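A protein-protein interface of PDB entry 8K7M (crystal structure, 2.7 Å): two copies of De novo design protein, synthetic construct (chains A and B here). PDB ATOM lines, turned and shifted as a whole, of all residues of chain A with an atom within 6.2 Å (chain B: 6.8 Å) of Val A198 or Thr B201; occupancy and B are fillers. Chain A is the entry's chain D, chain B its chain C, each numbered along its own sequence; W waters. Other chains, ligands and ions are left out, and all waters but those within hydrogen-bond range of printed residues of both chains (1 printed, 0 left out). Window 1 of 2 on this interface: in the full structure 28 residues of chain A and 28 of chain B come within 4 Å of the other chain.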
ATOM      1  N   ASN A 193       9.082 -11.461 -31.092  1.00  0.00           N
ATOM      2  CA  ASN A 193      10.133 -12.462 -31.028  1.00  0.00           C
ATOM      3  C   ASN A 193       9.983 -13.292 -29.755  1.00  0.00           C
ATOM      4  O   ASN A 193      10.055 -12.738 -28.652  1.00  0.00           O
ATOM      5  CB  ASN A 193      11.504 -11.783 -31.069  1.00  0.00           C
ATOM      6  CG  ASN A 193      12.649 -12.784 -31.037  1.00  0.00           C
ATOM      7  OD1 ASN A 193      13.012 -13.318 -29.979  1.00  0.00           O
ATOM      8  ND2 ASN A 193      13.206 -13.060 -32.197  1.00  0.00           N
ATOM      9  N   PRO A 194       9.770 -14.603 -29.856  1.00  0.00           N
ATOM     10  CA  PRO A 194       9.472 -15.373 -28.642  1.00  0.00           C
ATOM     11  C   PRO A 194      10.563 -15.297 -27.585  1.00  0.00           C
ATOM     12  O   PRO A 194      10.246 -15.308 -26.393  1.00  0.00           O
ATOM     13  CB  PRO A 194       9.288 -16.802 -29.177  1.00  0.00           C
ATOM     14  CG  PRO A 194       9.062 -16.656 -30.655  1.00  0.00           C
ATOM     15  CD  PRO A 194       9.854 -15.461 -31.051  1.00  0.00           C
ATOM     16  N   ALA A 195      11.840 -15.255 -27.975  1.00  0.00           N
ATOM     17  CA  ALA A 195      12.926 -15.188 -26.996  1.00  0.00           C
ATOM     18  C   ALA A 195      12.895 -13.861 -26.232  1.00  0.00           C
ATOM     19  O   ALA A 195      12.988 -13.830 -25.000  1.00  0.00           O
ATOM     20  CB  ALA A 195      14.271 -15.385 -27.694  1.00  0.00           C
ATOM     21  N   LEU A 196      12.749 -12.757 -26.958  1.00  0.00           N
ATOM     22  CA  LEU A 196      12.596 -11.466 -26.317  1.00  0.00           C
ATOM     23  C   LEU A 196      11.347 -11.435 -25.444  1.00  0.00           C
ATOM     24  O   LEU A 196      11.349 -10.841 -24.358  1.00  0.00           O
ATOM     25  CB  LEU A 196      12.542 -10.377 -27.386  1.00  0.00           C
ATOM     26  CG  LEU A 196      13.774 -10.258 -28.281  1.00  0.00           C
ATOM     27  CD1 LEU A 196      13.712  -8.954 -29.074  1.00  0.00           C
ATOM     28  CD2 LEU A 196      15.095 -10.412 -27.516  1.00  0.00           C
ATOM     29  N   ALA A 197      10.275 -12.079 -25.894  1.00  0.00           N
ATOM     30  CA  ALA A 197       9.051 -12.091 -25.107  1.00  0.00           C
ATOM     31  C   ALA A 197       9.241 -12.860 -23.802  1.00  0.00           C
ATOM     32  O   ALA A 197       8.780 -12.410 -22.747  1.00  0.00           O
ATOM     33  CB  ALA A 197       7.898 -12.651 -25.939  1.00  0.00           C
ATOM     34  N   VAL A 198       9.952 -13.995 -23.838  1.00  0.00           N
ATOM     35  CA  VAL A 198      10.206 -14.744 -22.604  1.00  0.00           C
ATOM     36  C   VAL A 198      11.060 -13.927 -21.648  1.00  0.00           C
ATOM     37  O   VAL A 198      10.743 -13.806 -20.459  1.00  0.00           O
ATOM     38  CB  VAL A 198      10.873 -16.096 -22.898  1.00  0.00           C
ATOM     39  CG1 VAL A 198      11.343 -16.695 -21.607  1.00  0.00           C
ATOM     40  CG2 VAL A 198       9.912 -17.024 -23.542  1.00  0.00           C
ATOM     41  N   GLU A 199      12.149 -13.345 -22.162  1.00  0.00           N
ATOM     42  CA  GLU A 199      13.049 -12.537 -21.339  1.00  0.00           C
ATOM     43  C   GLU A 199      12.317 -11.355 -20.688  1.00  0.00           C
ATOM     44  O   GLU A 199      12.465 -11.089 -19.481  1.00  0.00           O
ATOM     45  CB  GLU A 199      14.201 -12.054 -22.212  1.00  0.00           C
ATOM     46  CG  GLU A 199      15.323 -11.411 -21.457  1.00  0.00           C
ATOM     47  CD  GLU A 199      16.354 -10.781 -22.377  1.00  0.00           C
ATOM     48  OE1 GLU A 199      16.337 -11.066 -23.597  1.00  0.00           O
ATOM     49  OE2 GLU A 199      17.181  -9.989 -21.872  1.00  0.00           O
ATOM     50  N   VAL A 200      11.525 -10.626 -21.477  1.00  0.00           N
ATOM     51  CA  VAL A 200      10.847  -9.455 -20.957  1.00  0.00           C
ATOM     52  C   VAL A 200       9.753  -9.861 -19.984  1.00  0.00           C
ATOM     53  O   VAL A 200       9.509  -9.174 -18.994  1.00  0.00           O
ATOM     54  CB  VAL A 200      10.298  -8.599 -22.102  1.00  0.00           C
ATOM     55  CG1 VAL A 200       9.413  -7.485 -21.530  1.00  0.00           C
ATOM     56  CG2 VAL A 200      11.440  -8.036 -22.908  1.00  0.00           C
ATOM     57  N   THR A 201       9.045 -10.958 -20.255  1.00  0.00           N
ATOM     58  CA  THR A 201       8.087 -11.438 -19.268  1.00  0.00           C
ATOM     59  C   THR A 201       8.776 -11.745 -17.949  1.00  0.00           C
ATOM     60  O   THR A 201       8.287 -11.341 -16.885  1.00  0.00           O
ATOM     61  CB  THR A 201       7.328 -12.666 -19.796  1.00  0.00           C
ATOM     62  OG1 THR A 201       6.554 -12.277 -20.929  1.00  0.00           O
ATOM     63  CG2 THR A 201       6.394 -13.216 -18.750  1.00  0.00           C
ATOM     64  N   LYS A 202       9.919 -12.444 -17.998  1.00  0.00           N
ATOM     65  CA  LYS A 202      10.645 -12.767 -16.773  1.00  0.00           C
ATOM     66  C   LYS A 202      10.976 -11.493 -15.997  1.00  0.00           C
ATOM     67  O   LYS A 202      10.640 -11.355 -14.810  1.00  0.00           O
ATOM     68  CB  LYS A 202      11.915 -13.543 -17.122  1.00  0.00           C
ATOM     69  CG  LYS A 202      12.738 -13.990 -15.924  1.00  0.00           C
ATOM     70  CD  LYS A 202      13.954 -14.816 -16.338  1.00  0.00           C
ATOM     71  CE  LYS A 202      14.903 -15.029 -15.150  1.00  0.00           C
ATOM     72  NZ  LYS A 202      15.643 -13.797 -14.743  1.00  0.00           N
ATOM     73  N   PHE A 203      11.540 -10.509 -16.699  1.00  0.00           N
ATOM     74  CA  PHE A 203      11.873  -9.236 -16.076  1.00  0.00           C
ATOM     75  C   PHE A 203      10.634  -8.548 -15.471  1.00  0.00           C
ATOM     76  O   PHE A 203      10.654  -8.123 -14.309  1.00  0.00           O
ATOM     77  CB  PHE A 203      12.566  -8.359 -17.117  1.00  0.00           C
ATOM     78  CG  PHE A 203      12.714  -6.964 -16.698  1.00  0.00           C
ATOM     79  CD1 PHE A 203      13.697  -6.601 -15.794  1.00  0.00           C
ATOM     80  CD2 PHE A 203      11.856  -5.991 -17.197  1.00  0.00           C
ATOM     81  CE1 PHE A 203      13.845  -5.267 -15.381  1.00  0.00           C
ATOM     82  CE2 PHE A 203      11.984  -4.661 -16.794  1.00  0.00           C
ATOM     83  CZ  PHE A 203      12.988  -4.298 -15.875  1.00  0.00           C
ATOM     84  N   LEU A 205       7.640  -9.806 -14.494  1.00  0.00           N
ATOM     85  CA  LEU A 205       7.098 -10.492 -13.324  1.00  0.00           C
ATOM     86  C   LEU A 205       7.980 -10.278 -12.103  1.00  0.00           C
ATOM     87  O   LEU A 205       7.472 -10.101 -10.991  1.00  0.00           O
ATOM     88  CB  LEU A 205       6.943 -11.972 -13.612  1.00  0.00           C
ATOM     89  CG  LEU A 205       5.770 -12.206 -14.558  1.00  0.00           C
ATOM     90  CD1 LEU A 205       5.462 -13.690 -14.662  1.00  0.00           C
ATOM     91  CD2 LEU A 205       4.527 -11.408 -14.147  1.00  0.00           C
ATOM     92  N   MET B   3      17.126 -17.983 -16.348  1.00  0.00           N
ATOM     93  CA  MET B   3      16.803 -18.102 -17.757  1.00  0.00           C
ATOM     94  C   MET B   3      18.013 -18.673 -18.467  1.00  0.00           C
ATOM     95  O   MET B   3      19.118 -18.136 -18.351  1.00  0.00           O
ATOM     96  CB  MET B   3      16.406 -16.765 -18.375  1.00  0.00           C
ATOM     97  CG  MET B   3      15.699 -16.971 -19.697  1.00  0.00           C
ATOM     98  SD  MET B   3      15.599 -15.474 -20.660  1.00  0.00           S
ATOM     99  CE  MET B   3      15.487 -16.104 -22.318  1.00  0.00           C
ATOM    100  N   LEU B 187      11.552 -24.055 -24.331  1.00  0.00           N
ATOM    101  CA  LEU B 187      10.697 -23.635 -25.434  1.00  0.00           C
ATOM    102  C   LEU B 187      11.541 -23.145 -26.600  1.00  0.00           C
ATOM    103  O   LEU B 187      12.688 -22.738 -26.423  1.00  0.00           O
ATOM    104  CB  LEU B 187       9.768 -22.505 -24.993  1.00  0.00           C
ATOM    105  CG  LEU B 187       8.965 -22.767 -23.744  1.00  0.00           C
ATOM    106  CD1 LEU B 187       8.202 -21.495 -23.324  1.00  0.00           C
ATOM    107  CD2 LEU B 187       8.013 -23.865 -24.104  1.00  0.00           C
ATOM    108  N   SER B 188      10.953 -23.122 -27.794  1.00  0.00           N
ATOM    109  CA  SER B 188      11.659 -22.623 -28.971  1.00  0.00           C
ATOM    110  C   SER B 188      11.683 -21.091 -28.946  1.00  0.00           C
ATOM    111  O   SER B 188      10.639 -20.453 -28.832  1.00  0.00           O
ATOM    112  CB  SER B 188      10.996 -23.145 -30.243  1.00  0.00           C
ATOM    113  OG  SER B 188      11.608 -22.604 -31.405  1.00  0.00           O
ATOM    114  N   GLY B 189      12.866 -20.500 -28.960  1.00  0.00           N
ATOM    115  CA  GLY B 189      12.934 -19.050 -29.020  1.00  0.00           C
ATOM    116  C   GLY B 189      12.776 -18.466 -30.404  1.00  0.00           C
ATOM    117  O   GLY B 189      12.842 -17.247 -30.622  1.00  0.00           O
ATOM    118  N   PRO B 194       4.120 -16.439 -29.600  1.00  0.00           N
ATOM    119  CA  PRO B 194       4.586 -15.559 -28.516  1.00  0.00           C
ATOM    120  C   PRO B 194       3.601 -15.446 -27.370  1.00  0.00           C
ATOM    121  O   PRO B 194       4.033 -15.420 -26.213  1.00  0.00           O
ATOM    122  CB  PRO B 194       4.815 -14.224 -29.226  1.00  0.00           C
ATOM    123  CG  PRO B 194       4.899 -14.583 -30.675  1.00  0.00           C
ATOM    124  CD  PRO B 194       4.001 -15.731 -30.873  1.00  0.00           C
ATOM    125  N   LEU B 196       1.358 -17.745 -26.186  1.00  0.00           N
ATOM    126  CA  LEU B 196       1.530 -18.940 -25.362  1.00  0.00           C
ATOM    127  C   LEU B 196       2.856 -18.930 -24.622  1.00  0.00           C
ATOM    128  O   LEU B 196       2.936 -19.422 -23.495  1.00  0.00           O
ATOM    129  CB  LEU B 196       1.441 -20.206 -26.217  1.00  0.00           C
ATOM    130  CG  LEU B 196       0.121 -20.512 -26.924  1.00  0.00           C
ATOM    131  CD1 LEU B 196       0.172 -21.907 -27.472  1.00  0.00           C
ATOM    132  CD2 LEU B 196      -1.039 -20.360 -25.953  1.00  0.00           C
ATOM    133  N   ALA B 197       3.909 -18.398 -25.239  1.00  0.00           N
ATOM    134  CA  ALA B 197       5.206 -18.370 -24.580  1.00  0.00           C
ATOM    135  C   ALA B 197       5.158 -17.481 -23.355  1.00  0.00           C
ATOM    136  O   ALA B 197       5.716 -17.822 -22.307  1.00  0.00           O
ATOM    137  CB  ALA B 197       6.276 -17.896 -25.560  1.00  0.00           C
ATOM    138  N   VAL B 198       4.480 -16.336 -23.469  1.00  0.00           N
ATOM    139  CA  VAL B 198       4.342 -15.427 -22.341  1.00  0.00           C
ATOM    140  C   VAL B 198       3.555 -16.091 -21.229  1.00  0.00           C
ATOM    141  O   VAL B 198       3.964 -16.081 -20.063  1.00  0.00           O
ATOM    142  CB  VAL B 198       3.670 -14.123 -22.793  1.00  0.00           C
ATOM    143  CG1 VAL B 198       3.260 -13.301 -21.594  1.00  0.00           C
ATOM    144  CG2 VAL B 198       4.582 -13.344 -23.740  1.00  0.00           C
ATOM    145  N   GLU B 199       2.407 -16.685 -21.576  1.00  0.00           N
ATOM    146  CA  GLU B 199       1.599 -17.367 -20.566  1.00  0.00           C
ATOM    147  C   GLU B 199       2.386 -18.474 -19.866  1.00  0.00           C
ATOM    148  O   GLU B 199       2.333 -18.612 -18.637  1.00  0.00           O
ATOM    149  CB  GLU B 199       0.335 -17.943 -21.197  1.00  0.00           C
ATOM    150  CG  GLU B 199      -0.651 -18.483 -20.160  1.00  0.00           C
ATOM    151  CD  GLU B 199      -1.807 -19.232 -20.797  1.00  0.00           C
ATOM    152  OE1 GLU B 199      -1.972 -19.092 -22.028  1.00  0.00           O
ATOM    153  OE2 GLU B 199      -2.536 -19.965 -20.080  1.00  0.00           O
ATOM    154  N   VAL B 200       3.096 -19.302 -20.638  1.00  0.00           N
ATOM    155  CA  VAL B 200       3.791 -20.446 -20.056  1.00  0.00           C
ATOM    156  C   VAL B 200       4.968 -19.982 -19.215  1.00  0.00           C
ATOM    157  O   VAL B 200       5.251 -20.551 -18.157  1.00  0.00           O
ATOM    158  CB  VAL B 200       4.215 -21.433 -21.160  1.00  0.00           C
ATOM    159  CG1 VAL B 200       5.127 -22.518 -20.616  1.00  0.00           C
ATOM    160  CG2 VAL B 200       2.981 -22.055 -21.785  1.00  0.00           C
ATOM    161  N   THR B 201       5.673 -18.948 -19.664  1.00  0.00           N
ATOM    162  CA  THR B 201       6.718 -18.365 -18.841  1.00  0.00           C
ATOM    163  C   THR B 201       6.163 -17.874 -17.514  1.00  0.00           C
ATOM    164  O   THR B 201       6.756 -18.120 -16.457  1.00  0.00           O
ATOM    165  CB  THR B 201       7.400 -17.234 -19.601  1.00  0.00           C
ATOM    166  OG1 THR B 201       7.995 -17.781 -20.782  1.00  0.00           O
ATOM    167  CG2 THR B 201       8.480 -16.596 -18.748  1.00  0.00           C
ATOM    168  N   LYS B 202       5.030 -17.167 -17.549  1.00  0.00           N
ATOM    169  CA  LYS B 202       4.427 -16.677 -16.312  1.00  0.00           C
ATOM    170  C   LYS B 202       4.131 -17.826 -15.362  1.00  0.00           C
ATOM    171  O   LYS B 202       4.492 -17.791 -14.177  1.00  0.00           O
ATOM    172  CB  LYS B 202       3.155 -15.896 -16.625  1.00  0.00           C
ATOM    173  CG  LYS B 202       2.453 -15.333 -15.389  1.00  0.00           C
ATOM    174  CD  LYS B 202       1.274 -14.448 -15.753  1.00  0.00           C
ATOM    175  CE  LYS B 202       0.441 -14.106 -14.535  1.00  0.00           C
ATOM    176  NZ  LYS B 202      -0.363 -15.268 -14.070  1.00  0.00           N
ATOM    177  N   PHE B 203       3.501 -18.873 -15.885  1.00  0.00           N
ATOM    178  CA  PHE B 203       3.174 -20.028 -15.062  1.00  0.00           C
ATOM    179  C   PHE B 203       4.424 -20.670 -14.469  1.00  0.00           C
ATOM    180  O   PHE B 203       4.469 -20.970 -13.273  1.00  0.00           O
ATOM    181  CB  PHE B 203       2.386 -21.030 -15.892  1.00  0.00           C
ATOM    182  CG  PHE B 203       2.212 -22.342 -15.225  1.00  0.00           C
ATOM    183  CD1 PHE B 203       1.287 -22.491 -14.202  1.00  0.00           C
ATOM    184  CD2 PHE B 203       2.955 -23.444 -15.626  1.00  0.00           C
ATOM    185  CE1 PHE B 203       1.105 -23.723 -13.565  1.00  0.00           C
ATOM    186  CE2 PHE B 203       2.776 -24.685 -15.001  1.00  0.00           C
ATOM    187  CZ  PHE B 203       1.843 -24.822 -13.966  1.00  0.00           C
ATOM    188  N   LEU B 204       5.455 -20.886 -15.292  1.00  0.00           N
ATOM    189  CA  LEU B 204       6.672 -21.526 -14.803  1.00  0.00           C
ATOM    190  C   LEU B 204       7.332 -20.700 -13.712  1.00  0.00           C
ATOM    191  O   LEU B 204       7.702 -21.230 -12.656  1.00  0.00           O
ATOM    192  CB  LEU B 204       7.658 -21.757 -15.944  1.00  0.00           C
ATOM    193  CG  LEU B 204       7.210 -22.679 -17.074  1.00  0.00           C
ATOM    194  CD1 LEU B 204       8.286 -22.691 -18.130  1.00  0.00           C
ATOM    195  CD2 LEU B 204       6.924 -24.062 -16.556  1.00  0.00           C
ATOM    196  N   LEU B 205       7.518 -19.398 -13.956  1.00  0.00           N
ATOM    197  CA  LEU B 205       8.186 -18.559 -12.965  1.00  0.00           C
ATOM    198  C   LEU B 205       7.423 -18.554 -11.656  1.00  0.00           C
ATOM    199  O   LEU B 205       8.028 -18.635 -10.582  1.00  0.00           O
ATOM    200  CB  LEU B 205       8.321 -17.135 -13.478  1.00  0.00           C
ATOM    201  CG  LEU B 205       9.348 -16.897 -14.575  1.00  0.00           C
ATOM    202  CD1 LEU B 205       9.547 -15.405 -14.759  1.00  0.00           C
ATOM    203  CD2 LEU B 205      10.666 -17.609 -14.314  1.00  0.00           C
ATOM    204  N   GLU B 206       6.090 -18.510 -11.727  1.00  0.00           N
ATOM    205  CA  GLU B 206       5.292 -18.547 -10.506  1.00  0.00           C
ATOM    206  C   GLU B 206       5.499 -19.840  -9.734  1.00  0.00           C
ATOM    207  O   GLU B 206       5.420 -19.841  -8.505  1.00  0.00           O
ATOM    208  CB  GLU B 206       3.810 -18.338 -10.830  1.00  0.00           C
ATOM    209  CG  GLU B 206       3.479 -16.876 -11.116  1.00  0.00           C
ATOM    210  CD  GLU B 206       2.119 -16.669 -11.732  1.00  0.00           C
ATOM    211  OE1 GLU B 206       1.464 -17.670 -12.125  1.00  0.00           O
ATOM    212  OE2 GLU B 206       1.693 -15.487 -11.777  1.00  0.00           O
ATOM    213  N   LYS B 207       5.758 -20.950 -10.424  1.00  0.00           N
ATOM    214  CA  LYS B 207       6.040 -22.219  -9.768  1.00  0.00           C
ATOM    215  C   LYS B 207       7.512 -22.380  -9.392  1.00  0.00           C
ATOM    216  O   LYS B 207       7.916 -23.468  -8.972  1.00  0.00           O
ATOM    217  CB  LYS B 207       5.615 -23.378 -10.667  1.00  0.00           C
ATOM    218  CG  LYS B 207       4.138 -23.429 -11.001  1.00  0.00           C
ATOM    219  CD  LYS B 207       3.331 -24.006  -9.856  1.00  0.00           C
ATOM    220  CE  LYS B 207       1.846 -24.000 -10.184  1.00  0.00           C
ATOM    221  NZ  LYS B 207       1.009 -24.724  -9.173  1.00  0.00           N
ATOM    222  N   ILE B 209       9.990 -22.422 -11.460  1.00  0.00           N
ATOM    223  CA  ILE B 209      10.651 -23.207 -12.503  1.00  0.00           C
ATOM    224  C   ILE B 209      11.380 -22.288 -13.476  1.00  0.00           C
ATOM    225  O   ILE B 209      10.881 -21.223 -13.851  1.00  0.00           O
ATOM    226  CB  ILE B 209       9.647 -24.091 -13.260  1.00  0.00           C
ATOM    227  CG1 ILE B 209       8.944 -25.020 -12.287  1.00  0.00           C
ATOM    228  CG2 ILE B 209      10.362 -24.912 -14.329  1.00  0.00           C
ATOM    229  CD1 ILE B 209       7.720 -25.646 -12.888  1.00  0.00           C
ATOM    230  N   VAL B 211      13.125 -21.178 -17.129  1.00  0.00           N
ATOM    231  CA  VAL B 211      12.789 -21.198 -18.549  1.00  0.00           C
ATOM    232  C   VAL B 211      14.065 -21.288 -19.383  1.00  0.00           C
ATOM    233  O   VAL B 211      14.998 -20.497 -19.196  1.00  0.00           O
ATOM    234  CB  VAL B 211      11.979 -19.961 -18.947  1.00  0.00           C
ATOM    235  CG1 VAL B 211      11.445 -20.153 -20.347  1.00  0.00           C
ATOM    236  CG2 VAL B 211      10.877 -19.751 -17.963  1.00  0.00           C
ATOM    237  N   GLY B 212      14.087 -22.220 -20.327  1.00  0.00           N
ATOM    238  CA  GLY B 212      15.180 -22.358 -21.282  1.00  0.00           C
ATOM    239  C   GLY B 212      14.672 -22.014 -22.671  1.00  0.00           C
ATOM    240  O   GLY B 212      13.562 -22.398 -23.045  1.00  0.00           O
ATOM    241  N   VAL B 213      15.457 -21.250 -23.412  1.00  0.00           N
ATOM    242  CA  VAL B 213      15.063 -20.798 -24.736  1.00  0.00           C
ATOM    243  C   VAL B 213      15.993 -21.428 -25.767  1.00  0.00           C
ATOM    244  O   VAL B 213      17.212 -21.236 -25.705  1.00  0.00           O
ATOM    245  CB  VAL B 213      15.073 -19.269 -24.796  1.00  0.00           C
ATOM    246  CG1 VAL B 213      14.898 -18.786 -26.225  1.00  0.00           C
ATOM    247  CG2 VAL B 213      13.958 -18.730 -23.880  1.00  0.00           C
HETATM  248  O   HOH W   1      14.482 -15.409 -32.280  1.00  0.00           O
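Val A198 touches Thr B201, and with the chains exchanged Thr A201 touches Val B198.
Thr A201 touches its own counterpart, Thr B201.
Lys A202 touches Leu B205, and with the chains exchanged Leu A205 touches Lys B202.
The side-chain hydroxyl of Thr A201 lies within hydrogen-bond range of the backbone carbonyl oxygen of Ala A197 (2.9 Å).
The side-chain amide oxygen of Asn A193 is in hydrogen-bond range of the backbone NH of Leu A196 (3.1 Å).
The side-chain amide oxygen (OD1) of Asn A193 lies within hydrogen-bond range of the backbone NH (N) of Ala A195 (3.0 Å).
The side-chain amino group of Lys B202 is in salt-bridge range of the side-chain carboxylate of Glu B206 (3.1 Å).
O of Ala B197 is in hydrogen-bond range of OG1 of Thr B201, 2.7 Å away.
Among the printed residues, pairs that only touch across the chains: Val A198 with Thr B201 (3.4 Å), Lys A202 with Leu B205 (3.5 Å), Leu A205 with Lys B202 (3.5 Å), Pro A194 with Gly B189 (3.5 Å), Thr A201 with Val B198 (3.5 Å), Val A198 with Val B211 (3.7 Å), Lys A202 with Met B3 (3.7 Å), Ala A195 with Val B213 (3.8 Å), Pro A194 with Ser B188 (3.9 Å), Glu A199 with Met B3 (3.9 Å), Thr A201 with Thr B201 (3.97 Å) and Asn A193 with Gly B189 (3.98 Å).
Water W1 bridges the side-chain amide nitrogen of Asn A193 (2.7 Å) and the backbone carbonyl oxygen of Gly B189 (3.0 Å).
Hydrophobic or aromatic side chains of chain A that line the printed part of chain B: Pro A194, Ala A195, Val A198 and Leu A205.
Along chain A the printed residues that touch a printed residue of chain B span positions 193 to 205.
Printed residues of chain B that touch a printed residue of chain A: Met B3, Ser B188, Gly B189, Val B198, Thr B201, Lys B202, Leu B205, Val B211 and Val B213.
Among the printed residues, 13 pairs touch across the chains.
Among the printed residues, no Asp or Glu carboxylate lies within 4 Å of a Lys or Arg side-chain nitrogen of the other chain.
Of the printed residues of chain B, Val A198 touches Thr B201 and Val B211.
Of chain A, only Val A198 and Thr A201 come within 4 Å of Thr B201.
Of the printed residues of chain B, Pro A194 touches Ser B188 and Gly B189.
Of the printed residues of chain A, Val B198 touches Thr A201 (3.5 Å).
Ala B197 touches none of the printed residues of chain A.
Glu B206 touches none of the printed residues of chain A.
The nearest printed residue of chain B that does not touch Val A198 is Val B213 (4.02 Å).
The nearest printed residue of chain B that does not touch Ala A195 is Met B3 (4.3 Å).
N of Ala A195 lies within hydrogen-bond range of O of Gly B189.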
